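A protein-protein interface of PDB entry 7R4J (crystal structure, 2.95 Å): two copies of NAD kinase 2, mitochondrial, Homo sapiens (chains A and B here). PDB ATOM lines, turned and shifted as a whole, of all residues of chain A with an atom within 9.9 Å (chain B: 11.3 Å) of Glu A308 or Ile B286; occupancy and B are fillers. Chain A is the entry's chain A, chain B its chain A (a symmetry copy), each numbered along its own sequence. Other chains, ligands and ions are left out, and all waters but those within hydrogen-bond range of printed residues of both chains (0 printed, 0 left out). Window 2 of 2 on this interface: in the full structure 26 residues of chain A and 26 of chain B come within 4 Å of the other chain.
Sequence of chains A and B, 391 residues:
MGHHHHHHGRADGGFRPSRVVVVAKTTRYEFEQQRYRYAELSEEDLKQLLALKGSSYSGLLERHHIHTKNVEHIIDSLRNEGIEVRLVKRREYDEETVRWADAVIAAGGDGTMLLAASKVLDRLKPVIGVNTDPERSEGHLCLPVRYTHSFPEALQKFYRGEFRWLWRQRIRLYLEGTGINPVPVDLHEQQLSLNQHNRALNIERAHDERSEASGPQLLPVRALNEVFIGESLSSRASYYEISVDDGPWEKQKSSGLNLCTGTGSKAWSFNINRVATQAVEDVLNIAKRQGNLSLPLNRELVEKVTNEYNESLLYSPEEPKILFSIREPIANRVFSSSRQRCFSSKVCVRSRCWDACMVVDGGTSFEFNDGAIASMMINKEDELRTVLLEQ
OD2 of Asp B282 lies within salt-bridge range of NH2 of Arg A341 (3.8 Å).
The guanidinium group (NH2) of Arg A341 is in hydrogen-bond range of the side-chain hydroxyl (OH) of Tyr A309, at 2.8 Å.
O of Tyr A309 sits at hydrogen-bond distance from OG of Ser A312 (3.0 Å).
Among the printed residues, merely in contact across the chains: Tyr A309 with Ala B279, Tyr A309 with Asp B282, Glu A308 with Ile B286 and Val A305 with Ile B286.
Glu A308 touches just one residue of chain B: Ile B286 (3.5 Å).
Ile B286 touches two residues of chain A.
No residue of chain B comes within 4 Å of Lys A304.
Val A305 touches one residue of chain B.
No residue of chain B comes within 4 Å of Asn A307.
No residue of chain B comes within 4 Å of Asn A310.
No residue of chain B comes within 4 Å of Glu A311.
Asn B285 touches none of the printed residues of chain A.
No residue of chain A comes within 4 Å of Ala B287.
Arg B289 touches none of the printed residues of chain A.
Of the printed residues of chain B, Tyr A309 touches Ala B279 and Asp B282.
Of the printed residues of chain A, Asp B282 touches Tyr A309 and Arg A341.
Printed residues of chain B within 4 Å of Arg A341: Asp B282.
The nearest residue of chain B that does not touch Glu A308 is Arg B289 (5.8 Å).
The nearest residue of chain A that does not touch Ile B286 is Lys A304 (5.0 Å).
The nearest printed residue of chain B that does not touch Tyr A309 is Val B283 (4.3 Å).
Printed residues of chain B that touch a printed residue of chain A: Ala B279, Asp B282 and Ile B286.
Hydrophobic or aromatic side chains of chain B that line the printed part of chain A: Ala B279 and Ile B286.
Hydrophobic or aromatic side chains of chain A within 4 Å of the printed part of chain B: Tyr A309.
Among the printed residues, Asp or Glu carboxylates within 4 Å of a Lys or Arg side-chain nitrogen of the other chain: Arg A341 with Asp B282.
3 positions are printed for both chains.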
ATOM      1  N   PHE A 270     -21.873  28.618 -10.108  1.00  0.00           N
ATOM      2  CA  PHE A 270     -20.642  27.942 -10.518  1.00  0.00           C
ATOM      3  C   PHE A 270     -20.572  26.505  -9.976  1.00  0.00           C
ATOM      4  O   PHE A 270     -20.415  25.545 -10.746  1.00  0.00           O
ATOM      5  CB  PHE A 270     -19.435  28.783 -10.058  1.00  0.00           C
ATOM      6  CG  PHE A 270     -18.108  28.314 -10.604  1.00  0.00           C
ATOM      7  CD1 PHE A 270     -17.710  28.662 -11.881  1.00  0.00           C
ATOM      8  CD2 PHE A 270     -17.255  27.539  -9.837  1.00  0.00           C
ATOM      9  CE1 PHE A 270     -16.505  28.229 -12.388  1.00  0.00           C
ATOM     10  CE2 PHE A 270     -16.047  27.113 -10.341  1.00  0.00           C
ATOM     11  CZ  PHE A 270     -15.671  27.460 -11.613  1.00  0.00           C
ATOM     12  N   ARG A 274     -20.224  23.581 -12.638  1.00  0.00           N
ATOM     13  CA  ARG A 274     -18.832  23.261 -12.941  1.00  0.00           C
ATOM     14  C   ARG A 274     -18.617  21.754 -13.103  1.00  0.00           C
ATOM     15  O   ARG A 274     -19.367  20.928 -12.564  1.00  0.00           O
ATOM     16  CB  ARG A 274     -17.928  23.814 -11.841  1.00  0.00           C
ATOM     17  CG  ARG A 274     -18.035  23.081 -10.512  1.00  0.00           C
ATOM     18  CD  ARG A 274     -16.830  23.368  -9.654  1.00  0.00           C
ATOM     19  NE  ARG A 274     -15.654  22.741 -10.228  1.00  0.00           N
ATOM     20  CZ  ARG A 274     -14.805  22.010  -9.526  1.00  0.00           C
ATOM     21  NH1 ARG A 274     -14.976  21.815  -8.227  1.00  0.00           N
ATOM     22  NH2 ARG A 274     -13.764  21.456 -10.142  1.00  0.00           N
ATOM     23  N   VAL A 275     -17.583  21.403 -13.872  1.00  0.00           N
ATOM     24  CA  VAL A 275     -17.171  20.013 -14.045  1.00  0.00           C
ATOM     25  C   VAL A 275     -15.922  19.758 -13.216  1.00  0.00           C
ATOM     26  O   VAL A 275     -15.234  20.680 -12.767  1.00  0.00           O
ATOM     27  CB  VAL A 275     -16.910  19.624 -15.519  1.00  0.00           C
ATOM     28  CG1 VAL A 275     -18.209  19.533 -16.275  1.00  0.00           C
ATOM     29  CG2 VAL A 275     -15.933  20.599 -16.182  1.00  0.00           C
ATOM     30  N   THR A 277     -12.171  17.659 -12.845  1.00  0.00           N
ATOM     31  CA  THR A 277     -11.110  17.166 -13.711  1.00  0.00           C
ATOM     32  C   THR A 277     -10.947  15.653 -13.624  1.00  0.00           C
ATOM     33  O   THR A 277     -10.422  15.049 -14.564  1.00  0.00           O
ATOM     34  CB  THR A 277      -9.793  17.864 -13.382  1.00  0.00           C
ATOM     35  OG1 THR A 277      -9.522  17.745 -11.977  1.00  0.00           O
ATOM     36  CG2 THR A 277      -9.883  19.341 -13.760  1.00  0.00           C
ATOM     37  N   VAL A 280     -13.816  14.308 -16.106  1.00  0.00           N
ATOM     38  CA  VAL A 280     -13.632  14.479 -17.549  1.00  0.00           C
ATOM     39  C   VAL A 280     -12.676  13.421 -18.098  1.00  0.00           C
ATOM     40  O   VAL A 280     -12.840  12.968 -19.235  1.00  0.00           O
ATOM     41  CB  VAL A 280     -13.139  15.895 -17.907  1.00  0.00           C
ATOM     42  CG1 VAL A 280     -14.281  16.899 -17.892  1.00  0.00           C
ATOM     43  CG2 VAL A 280     -12.016  16.338 -16.987  1.00  0.00           C
ATOM     44  N   LEU A 284     -13.672  11.275 -21.026  1.00  0.00           N
ATOM     45  CA  LEU A 284     -12.882  11.269 -22.245  1.00  0.00           C
ATOM     46  C   LEU A 284     -12.259   9.904 -22.534  1.00  0.00           C
ATOM     47  O   LEU A 284     -11.732   9.693 -23.637  1.00  0.00           O
ATOM     48  CB  LEU A 284     -11.803  12.357 -22.160  1.00  0.00           C
ATOM     49  CG  LEU A 284     -11.678  13.344 -23.322  1.00  0.00           C
ATOM     50  CD1 LEU A 284     -13.062  13.744 -23.842  1.00  0.00           C
ATOM     51  CD2 LEU A 284     -10.906  14.563 -22.859  1.00  0.00           C
ATOM     52  N   LEU A 295      -6.704  12.485 -29.736  1.00  0.00           N
ATOM     53  CA  LEU A 295      -5.722  12.894 -28.749  1.00  0.00           C
ATOM     54  C   LEU A 295      -5.117  11.690 -28.040  1.00  0.00           C
ATOM     55  O   LEU A 295      -5.747  10.627 -27.939  1.00  0.00           O
ATOM     56  CB  LEU A 295      -6.357  13.824 -27.715  1.00  0.00           C
ATOM     57  N   GLU A 300      -2.125  17.710 -19.045  1.00  0.00           N
ATOM     58  CA  GLU A 300      -2.207  19.107 -19.465  1.00  0.00           C
ATOM     59  C   GLU A 300      -3.508  19.384 -20.209  1.00  0.00           C
ATOM     60  O   GLU A 300      -4.086  20.472 -20.076  1.00  0.00           O
ATOM     61  CB  GLU A 300      -0.992  19.461 -20.339  1.00  0.00           C
ATOM     62  CG  GLU A 300      -0.768  20.959 -20.593  1.00  0.00           C
ATOM     63  CD  GLU A 300       0.684  21.393 -20.408  1.00  0.00           C
ATOM     64  OE1 GLU A 300       1.455  21.320 -21.390  1.00  0.00           O
ATOM     65  OE2 GLU A 300       1.052  21.825 -19.293  1.00  0.00           O
ATOM     66  N   LEU A 301      -3.987  18.409 -20.982  1.00  0.00           N
ATOM     67  CA  LEU A 301      -5.237  18.591 -21.709  1.00  0.00           C
ATOM     68  C   LEU A 301      -6.434  18.519 -20.765  1.00  0.00           C
ATOM     69  O   LEU A 301      -7.374  19.313 -20.895  1.00  0.00           O
ATOM     70  CB  LEU A 301      -5.329  17.551 -22.830  1.00  0.00           C
ATOM     71  CG  LEU A 301      -6.210  17.827 -24.051  1.00  0.00           C
ATOM     72  CD1 LEU A 301      -7.688  17.741 -23.717  1.00  0.00           C
ATOM     73  CD2 LEU A 301      -5.881  19.175 -24.654  1.00  0.00           C
ATOM     74  N   VAL A 302      -6.397  17.600 -19.784  1.00  0.00           N
ATOM     75  CA  VAL A 302      -7.516  17.411 -18.854  1.00  0.00           C
ATOM     76  C   VAL A 302      -7.894  18.723 -18.183  1.00  0.00           C
ATOM     77  O   VAL A 302      -9.070  18.976 -17.888  1.00  0.00           O
ATOM     78  CB  VAL A 302      -7.173  16.339 -17.803  1.00  0.00           C
ATOM     79  CG1 VAL A 302      -8.445  15.802 -17.183  1.00  0.00           C
ATOM     80  CG2 VAL A 302      -6.371  15.209 -18.411  1.00  0.00           C
ATOM     81  N   GLU A 303      -6.899  19.568 -17.917  1.00  0.00           N
ATOM     82  CA  GLU A 303      -7.176  20.865 -17.329  1.00  0.00           C
ATOM     83  C   GLU A 303      -7.615  21.881 -18.381  1.00  0.00           C
ATOM     84  O   GLU A 303      -8.383  22.797 -18.064  1.00  0.00           O
ATOM     85  CB  GLU A 303      -5.942  21.368 -16.571  1.00  0.00           C
ATOM     86  CG  GLU A 303      -5.925  21.153 -15.037  1.00  0.00           C
ATOM     87  CD  GLU A 303      -7.048  21.859 -14.246  1.00  0.00           C
ATOM     88  OE1 GLU A 303      -8.069  22.312 -14.821  1.00  0.00           O
ATOM     89  OE2 GLU A 303      -6.890  21.965 -13.007  1.00  0.00           O
ATOM     90  N   LYS A 304      -7.169  21.736 -19.631  1.00  0.00           N
ATOM     91  CA  LYS A 304      -7.487  22.748 -20.631  1.00  0.00           C
ATOM     92  C   LYS A 304      -8.828  22.511 -21.316  1.00  0.00           C
ATOM     93  O   LYS A 304      -9.306  23.404 -22.023  1.00  0.00           O
ATOM     94  CB  LYS A 304      -6.353  22.856 -21.666  1.00  0.00           C
ATOM     95  CG  LYS A 304      -6.615  22.277 -23.043  1.00  0.00           C
ATOM     96  CD  LYS A 304      -5.633  22.872 -24.041  1.00  0.00           C
ATOM     97  CE  LYS A 304      -5.840  24.381 -24.168  1.00  0.00           C
ATOM     98  NZ  LYS A 304      -4.906  25.021 -25.135  1.00  0.00           N
ATOM     99  N   VAL A 305      -9.460  21.361 -21.096  1.00  0.00           N
ATOM    100  CA  VAL A 305     -10.850  21.178 -21.502  1.00  0.00           C
ATOM    101  C   VAL A 305     -11.808  21.583 -20.391  1.00  0.00           C
ATOM    102  O   VAL A 305     -12.875  22.139 -20.662  1.00  0.00           O
ATOM    103  CB  VAL A 305     -11.103  19.728 -21.946  1.00  0.00           C
ATOM    104  CG1 VAL A 305     -10.655  19.530 -23.386  1.00  0.00           C
ATOM    105  CG2 VAL A 305     -10.418  18.754 -20.996  1.00  0.00           C
ATOM    106  N   THR A 306     -11.463  21.310 -19.130  1.00  0.00           N
ATOM    107  CA  THR A 306     -12.302  21.782 -18.030  1.00  0.00           C
ATOM    108  C   THR A 306     -12.247  23.301 -17.899  1.00  0.00           C
ATOM    109  O   THR A 306     -13.280  23.943 -17.680  1.00  0.00           O
ATOM    110  CB  THR A 306     -11.890  21.122 -16.711  1.00  0.00           C
ATOM    111  OG1 THR A 306     -10.468  20.979 -16.659  1.00  0.00           O
ATOM    112  CG2 THR A 306     -12.514  19.768 -16.583  1.00  0.00           C
ATOM    113  N   ASN A 307     -11.056  23.895 -18.041  1.00  0.00           N
ATOM    114  CA  ASN A 307     -10.889  25.325 -17.808  1.00  0.00           C
ATOM    115  C   ASN A 307     -11.533  26.182 -18.880  1.00  0.00           C
ATOM    116  O   ASN A 307     -11.814  27.356 -18.620  1.00  0.00           O
ATOM    117  CB  ASN A 307      -9.415  25.676 -17.706  1.00  0.00           C
ATOM    118  CG  ASN A 307      -8.883  25.463 -16.327  1.00  0.00           C
ATOM    119  OD1 ASN A 307      -9.522  24.805 -15.507  1.00  0.00           O
ATOM    120  ND2 ASN A 307      -7.705  26.003 -16.054  1.00  0.00           N
ATOM    121  N   GLU A 308     -11.755  25.646 -20.076  1.00  0.00           N
ATOM    122  CA  GLU A 308     -12.531  26.386 -21.057  1.00  0.00           C
ATOM    123  C   GLU A 308     -14.028  26.130 -20.917  1.00  0.00           C
ATOM    124  O   GLU A 308     -14.827  26.963 -21.368  1.00  0.00           O
ATOM    125  CB  GLU A 308     -12.042  26.052 -22.474  1.00  0.00           C
ATOM    126  CG  GLU A 308     -10.535  26.314 -22.686  1.00  0.00           C
ATOM    127  CD  GLU A 308     -10.199  26.920 -24.048  1.00  0.00           C
ATOM    128  OE1 GLU A 308     -10.742  28.001 -24.374  1.00  0.00           O
ATOM    129  OE2 GLU A 308      -9.379  26.322 -24.786  1.00  0.00           O
ATOM    130  N   TYR A 309     -14.421  25.018 -20.271  1.00  0.00           N
ATOM    131  CA  TYR A 309     -15.834  24.775 -19.966  1.00  0.00           C
ATOM    132  C   TYR A 309     -16.318  25.658 -18.822  1.00  0.00           C
ATOM    133  O   TYR A 309     -17.331  26.357 -18.949  1.00  0.00           O
ATOM    134  CB  TYR A 309     -16.083  23.309 -19.608  1.00  0.00           C
ATOM    135  CG  TYR A 309     -17.562  22.982 -19.634  1.00  0.00           C
ATOM    136  CD1 TYR A 309     -18.232  22.576 -18.482  1.00  0.00           C
ATOM    137  CD2 TYR A 309     -18.302  23.107 -20.806  1.00  0.00           C
ATOM    138  CE1 TYR A 309     -19.603  22.287 -18.505  1.00  0.00           C
ATOM    139  CE2 TYR A 309     -19.667  22.817 -20.836  1.00  0.00           C
ATOM    140  CZ  TYR A 309     -20.312  22.405 -19.692  1.00  0.00           C
ATOM    141  OH  TYR A 309     -21.661  22.124 -19.746  1.00  0.00           O
ATOM    142  N   ASN A 310     -15.628  25.601 -17.679  1.00  0.00           N
ATOM    143  CA  ASN A 310     -15.963  26.452 -16.548  1.00  0.00           C
ATOM    144  C   ASN A 310     -15.862  27.929 -16.901  1.00  0.00           C
ATOM    145  O   ASN A 310     -16.444  28.762 -16.199  1.00  0.00           O
ATOM    146  CB  ASN A 310     -15.048  26.128 -15.359  1.00  0.00           C
ATOM    147  CG  ASN A 310     -15.114  24.652 -14.940  1.00  0.00           C
ATOM    148  OD1 ASN A 310     -16.082  23.937 -15.249  1.00  0.00           O
ATOM    149  ND2 ASN A 310     -14.071  24.192 -14.237  1.00  0.00           N
ATOM    150  N   GLU A 311     -15.150  28.270 -17.984  1.00  0.00           N
ATOM    151  CA  GLU A 311     -15.010  29.656 -18.413  1.00  0.00           C
ATOM    152  C   GLU A 311     -16.257  30.202 -19.097  1.00  0.00           C
ATOM    153  O   GLU A 311     -16.432  31.426 -19.146  1.00  0.00           O
ATOM    154  CB  GLU A 311     -13.811  29.808 -19.355  1.00  0.00           C
ATOM    155  CG  GLU A 311     -12.523  30.221 -18.659  1.00  0.00           C
ATOM    156  CD  GLU A 311     -12.696  31.430 -17.758  1.00  0.00           C
ATOM    157  OE1 GLU A 311     -13.436  32.368 -18.134  1.00  0.00           O
ATOM    158  OE2 GLU A 311     -12.095  31.435 -16.661  1.00  0.00           O
ATOM    159  N   SER A 312     -17.119  29.341 -19.629  1.00  0.00           N
ATOM    160  CA  SER A 312     -18.356  29.815 -20.235  1.00  0.00           C
ATOM    161  C   SER A 312     -19.480  30.011 -19.225  1.00  0.00           C
ATOM    162  O   SER A 312     -20.497  30.625 -19.570  1.00  0.00           O
ATOM    163  CB  SER A 312     -18.811  28.854 -21.336  1.00  0.00           C
ATOM    164  OG  SER A 312     -19.346  27.667 -20.784  1.00  0.00           O
ATOM    165  N   LEU A 313     -19.322  29.520 -17.992  1.00  0.00           N
ATOM    166  CA  LEU A 313     -20.314  29.690 -16.934  1.00  0.00           C
ATOM    167  C   LEU A 313     -20.230  31.032 -16.229  1.00  0.00           C
ATOM    168  O   LEU A 313     -20.997  31.251 -15.285  1.00  0.00           O
ATOM    169  CB  LEU A 313     -20.172  28.615 -15.860  1.00  0.00           C
ATOM    170  CG  LEU A 313     -20.161  27.133 -16.165  1.00  0.00           C
ATOM    171  CD1 LEU A 313     -19.521  26.415 -14.986  1.00  0.00           C
ATOM    172  CD2 LEU A 313     -21.571  26.655 -16.420  1.00  0.00           C
ATOM    173  N   LEU A 314     -19.297  31.901 -16.617  1.00  0.00           N
ATOM    174  CA  LEU A 314     -19.140  33.224 -16.019  1.00  0.00           C
ATOM    175  C   LEU A 314     -19.399  34.283 -17.078  1.00  0.00           C
ATOM    176  O   LEU A 314     -18.877  34.191 -18.194  1.00  0.00           O
ATOM    177  CB  LEU A 314     -17.739  33.448 -15.436  1.00  0.00           C
ATOM    178  CG  LEU A 314     -16.986  32.382 -14.651  1.00  0.00           C
ATOM    179  CD1 LEU A 314     -15.797  33.016 -13.947  1.00  0.00           C
ATOM    180  CD2 LEU A 314     -17.909  31.734 -13.643  1.00  0.00           C
ATOM    181  N   ARG A 341     -29.323  24.667 -18.225  1.00  0.00           N
ATOM    182  CA  ARG A 341     -29.190  26.086 -17.910  1.00  0.00           C
ATOM    183  C   ARG A 341     -29.288  26.867 -19.216  1.00  0.00           C
ATOM    184  O   ARG A 341     -29.180  26.297 -20.304  1.00  0.00           O
ATOM    185  CB  ARG A 341     -27.871  26.404 -17.199  1.00  0.00           C
ATOM    186  CG  ARG A 341     -26.689  25.766 -17.846  1.00  0.00           C
ATOM    187  CD  ARG A 341     -25.487  26.659 -17.871  1.00  0.00           C
ATOM    188  NE  ARG A 341     -24.467  26.150 -18.783  1.00  0.00           N
ATOM    189  CZ  ARG A 341     -23.778  25.027 -18.608  1.00  0.00           C
ATOM    190  NH1 ARG A 341     -23.945  24.272 -17.532  1.00  0.00           N
ATOM    191  NH2 ARG A 341     -22.896  24.649 -19.538  1.00  0.00           N
ATOM    192  N   GLN B 278     -27.040  17.444 -22.892  1.00  0.00           N
ATOM    193  CA  GLN B 278     -26.847  18.778 -23.457  1.00  0.00           C
ATOM    194  C   GLN B 278     -25.532  19.412 -23.032  1.00  0.00           C
ATOM    195  O   GLN B 278     -25.122  20.410 -23.641  1.00  0.00           O
ATOM    196  CB  GLN B 278     -28.009  19.701 -23.064  1.00  0.00           C
ATOM    197  N   ALA B 279     -24.877  18.855 -22.010  1.00  0.00           N
ATOM    198  CA  ALA B 279     -23.605  19.351 -21.502  1.00  0.00           C
ATOM    199  C   ALA B 279     -22.447  18.398 -21.759  1.00  0.00           C
ATOM    200  O   ALA B 279     -21.330  18.678 -21.314  1.00  0.00           O
ATOM    201  CB  ALA B 279     -23.716  19.650 -20.001  1.00  0.00           C
ATOM    202  N   VAL B 280     -22.687  17.273 -22.439  1.00  0.00           N
ATOM    203  CA  VAL B 280     -21.597  16.516 -23.056  1.00  0.00           C
ATOM    204  C   VAL B 280     -21.334  17.011 -24.477  1.00  0.00           C
ATOM    205  O   VAL B 280     -20.186  17.011 -24.932  1.00  0.00           O
ATOM    206  CB  VAL B 280     -21.871  14.998 -23.052  1.00  0.00           C
ATOM    207  CG1 VAL B 280     -21.581  14.387 -21.691  1.00  0.00           C
ATOM    208  CG2 VAL B 280     -23.291  14.692 -23.492  1.00  0.00           C
ATOM    209  N   GLU B 281     -22.386  17.417 -25.193  1.00  0.00           N
ATOM    210  CA  GLU B 281     -22.209  18.192 -26.421  1.00  0.00           C
ATOM    211  C   GLU B 281     -21.377  19.439 -26.160  1.00  0.00           C
ATOM    212  O   GLU B 281     -20.539  19.820 -26.985  1.00  0.00           O
ATOM    213  CB  GLU B 281     -23.576  18.574 -26.992  1.00  0.00           C
ATOM    214  CG  GLU B 281     -23.548  19.449 -28.224  1.00  0.00           C
ATOM    215  CD  GLU B 281     -24.784  19.237 -29.076  1.00  0.00           C
ATOM    216  OE1 GLU B 281     -25.702  18.521 -28.615  1.00  0.00           O
ATOM    217  OE2 GLU B 281     -24.841  19.772 -30.207  1.00  0.00           O
ATOM    218  N   ASP B 282     -21.610  20.097 -25.018  1.00  0.00           N
ATOM    219  CA  ASP B 282     -20.808  21.256 -24.647  1.00  0.00           C
ATOM    220  C   ASP B 282     -19.370  20.843 -24.339  1.00  0.00           C
ATOM    221  O   ASP B 282     -18.425  21.562 -24.682  1.00  0.00           O
ATOM    222  CB  ASP B 282     -21.455  21.982 -23.459  1.00  0.00           C
ATOM    223  CG  ASP B 282     -22.370  23.149 -23.886  1.00  0.00           C
ATOM    224  OD1 ASP B 282     -23.156  22.988 -24.849  1.00  0.00           O
ATOM    225  OD2 ASP B 282     -22.312  24.229 -23.246  1.00  0.00           O
ATOM    226  N   VAL B 283     -19.176  19.670 -23.732  1.00  0.00           N
ATOM    227  CA  VAL B 283     -17.816  19.236 -23.409  1.00  0.00           C
ATOM    228  C   VAL B 283     -17.126  18.640 -24.635  1.00  0.00           C
ATOM    229  O   VAL B 283     -15.903  18.751 -24.775  1.00  0.00           O
ATOM    230  CB  VAL B 283     -17.797  18.245 -22.221  1.00  0.00           C
ATOM    231  CG1 VAL B 283     -18.176  16.836 -22.654  1.00  0.00           C
ATOM    232  CG2 VAL B 283     -16.428  18.230 -21.550  1.00  0.00           C
ATOM    233  N   LEU B 284     -17.868  18.019 -25.544  1.00  0.00           N
ATOM    234  CA  LEU B 284     -17.213  17.358 -26.660  1.00  0.00           C
ATOM    235  C   LEU B 284     -16.937  18.309 -27.824  1.00  0.00           C
ATOM    236  O   LEU B 284     -16.206  17.940 -28.756  1.00  0.00           O
ATOM    237  CB  LEU B 284     -18.061  16.164 -27.117  1.00  0.00           C
ATOM    238  CG  LEU B 284     -17.378  14.805 -27.263  1.00  0.00           C
ATOM    239  CD1 LEU B 284     -16.374  14.579 -26.129  1.00  0.00           C
ATOM    240  CD2 LEU B 284     -18.431  13.715 -27.271  1.00  0.00           C
ATOM    241  N   ASN B 285     -17.480  19.531 -27.774  1.00  0.00           N
ATOM    242  CA  ASN B 285     -17.258  20.537 -28.807  1.00  0.00           C
ATOM    243  C   ASN B 285     -16.069  21.432 -28.495  1.00  0.00           C
ATOM    244  O   ASN B 285     -15.420  21.932 -29.424  1.00  0.00           O
ATOM    245  CB  ASN B 285     -18.519  21.389 -28.989  1.00  0.00           C
ATOM    246  CG  ASN B 285     -19.446  20.827 -30.039  1.00  0.00           C
ATOM    247  OD1 ASN B 285     -19.009  20.117 -30.939  1.00  0.00           O
ATOM    248  ND2 ASN B 285     -20.737  21.127 -29.918  1.00  0.00           N
ATOM    249  N   ILE B 286     -15.788  21.664 -27.207  1.00  0.00           N
ATOM    250  CA  ILE B 286     -14.510  22.248 -26.804  1.00  0.00           C
ATOM    251  C   ILE B 286     -13.407  21.205 -26.940  1.00  0.00           C
ATOM    252  O   ILE B 286     -12.235  21.544 -27.162  1.00  0.00           O
ATOM    253  CB  ILE B 286     -14.603  22.811 -25.364  1.00  0.00           C
ATOM    254  CG1 ILE B 286     -14.688  24.361 -25.356  1.00  0.00           C
ATOM    255  CG2 ILE B 286     -13.487  22.246 -24.460  1.00  0.00           C
ATOM    256  CD1 ILE B 286     -13.378  25.128 -25.579  1.00  0.00           C
ATOM    257  N   ALA B 287     -13.770  19.923 -26.842  1.00  0.00           N
ATOM    258  CA  ALA B 287     -12.867  18.812 -27.112  1.00  0.00           C
ATOM    259  C   ALA B 287     -12.736  18.593 -28.615  1.00  0.00           C
ATOM    260  O   ALA B 287     -12.445  17.486 -29.080  1.00  0.00           O
ATOM    261  CB  ALA B 287     -13.369  17.544 -26.420  1.00  0.00           C
ATOM    262  N   LYS B 288     -12.966  19.653 -29.381  1.00  0.00           N
ATOM    263  CA  LYS B 288     -12.793  19.658 -30.822  1.00  0.00           C
ATOM    264  C   LYS B 288     -11.610  20.521 -31.238  1.00  0.00           C
ATOM    265  O   LYS B 288     -10.793  20.097 -32.061  1.00  0.00           O
ATOM    266  CB  LYS B 288     -14.092  20.150 -31.487  1.00  0.00           C
ATOM    267  CG  LYS B 288     -14.503  19.422 -32.747  1.00  0.00           C
ATOM    268  CD  LYS B 288     -15.862  19.911 -33.249  1.00  0.00           C
ATOM    269  CE  LYS B 288     -15.931  19.837 -34.787  1.00  0.00           C
ATOM    270  NZ  LYS B 288     -17.295  19.569 -35.338  1.00  0.00           N
ATOM    271  N   ARG B 289     -11.475  21.709 -30.656  1.00  0.00           N
ATOM    272  CA  ARG B 289     -10.326  22.573 -30.938  1.00  0.00           C
ATOM    273  C   ARG B 289      -9.082  22.101 -30.195  1.00  0.00           C
ATOM    274  O   ARG B 289      -8.669  22.722 -29.214  1.00  0.00           O
ATOM    275  CB  ARG B 289     -10.628  24.026 -30.559  1.00  0.00           C
ATOM    276  N   SER B 294     -11.357  13.078 -34.010  1.00  0.00           N
ATOM    277  CA  SER B 294     -11.720  11.698 -34.311  1.00  0.00           C
ATOM    278  C   SER B 294     -13.076  11.652 -34.986  1.00  0.00           C
ATOM    279  O   SER B 294     -13.200  11.423 -36.195  1.00  0.00           O
ATOM    280  CB  SER B 294     -11.781  10.829 -33.041  1.00  0.00           C
ATOM    281  OG  SER B 294     -10.683  11.011 -32.164  1.00  0.00           O
ATOM    282  N   LEU B 295     -14.124  11.871 -34.150  1.00  0.00           N
ATOM    283  CA  LEU B 295     -15.526  11.655 -34.460  1.00  0.00           C
ATOM    284  C   LEU B 295     -16.124  12.856 -35.180  1.00  0.00           C
ATOM    285  O   LEU B 295     -15.652  13.992 -35.024  1.00  0.00           O
ATOM    286  CB  LEU B 295     -16.320  11.383 -33.182  1.00  0.00           C
ATOM    287  N   LEU B 297     -19.339  13.461 -34.519  1.00  0.00           N
ATOM    288  CA  LEU B 297     -20.288  13.847 -33.473  1.00  0.00           C
ATOM    289  C   LEU B 297     -21.737  13.921 -33.967  1.00  0.00           C
ATOM    290  O   LEU B 297     -22.215  14.992 -34.359  1.00  0.00           O
ATOM    291  CB  LEU B 297     -19.876  15.186 -32.832  1.00  0.00           C
ATOM    292  CG  LEU B 297     -18.671  15.254 -31.865  1.00  0.00           C
ATOM    293  CD1 LEU B 297     -17.335  15.015 -32.570  1.00  0.00           C
ATOM    294  CD2 LEU B 297     -18.622  16.568 -31.065  1.00  0.00           C
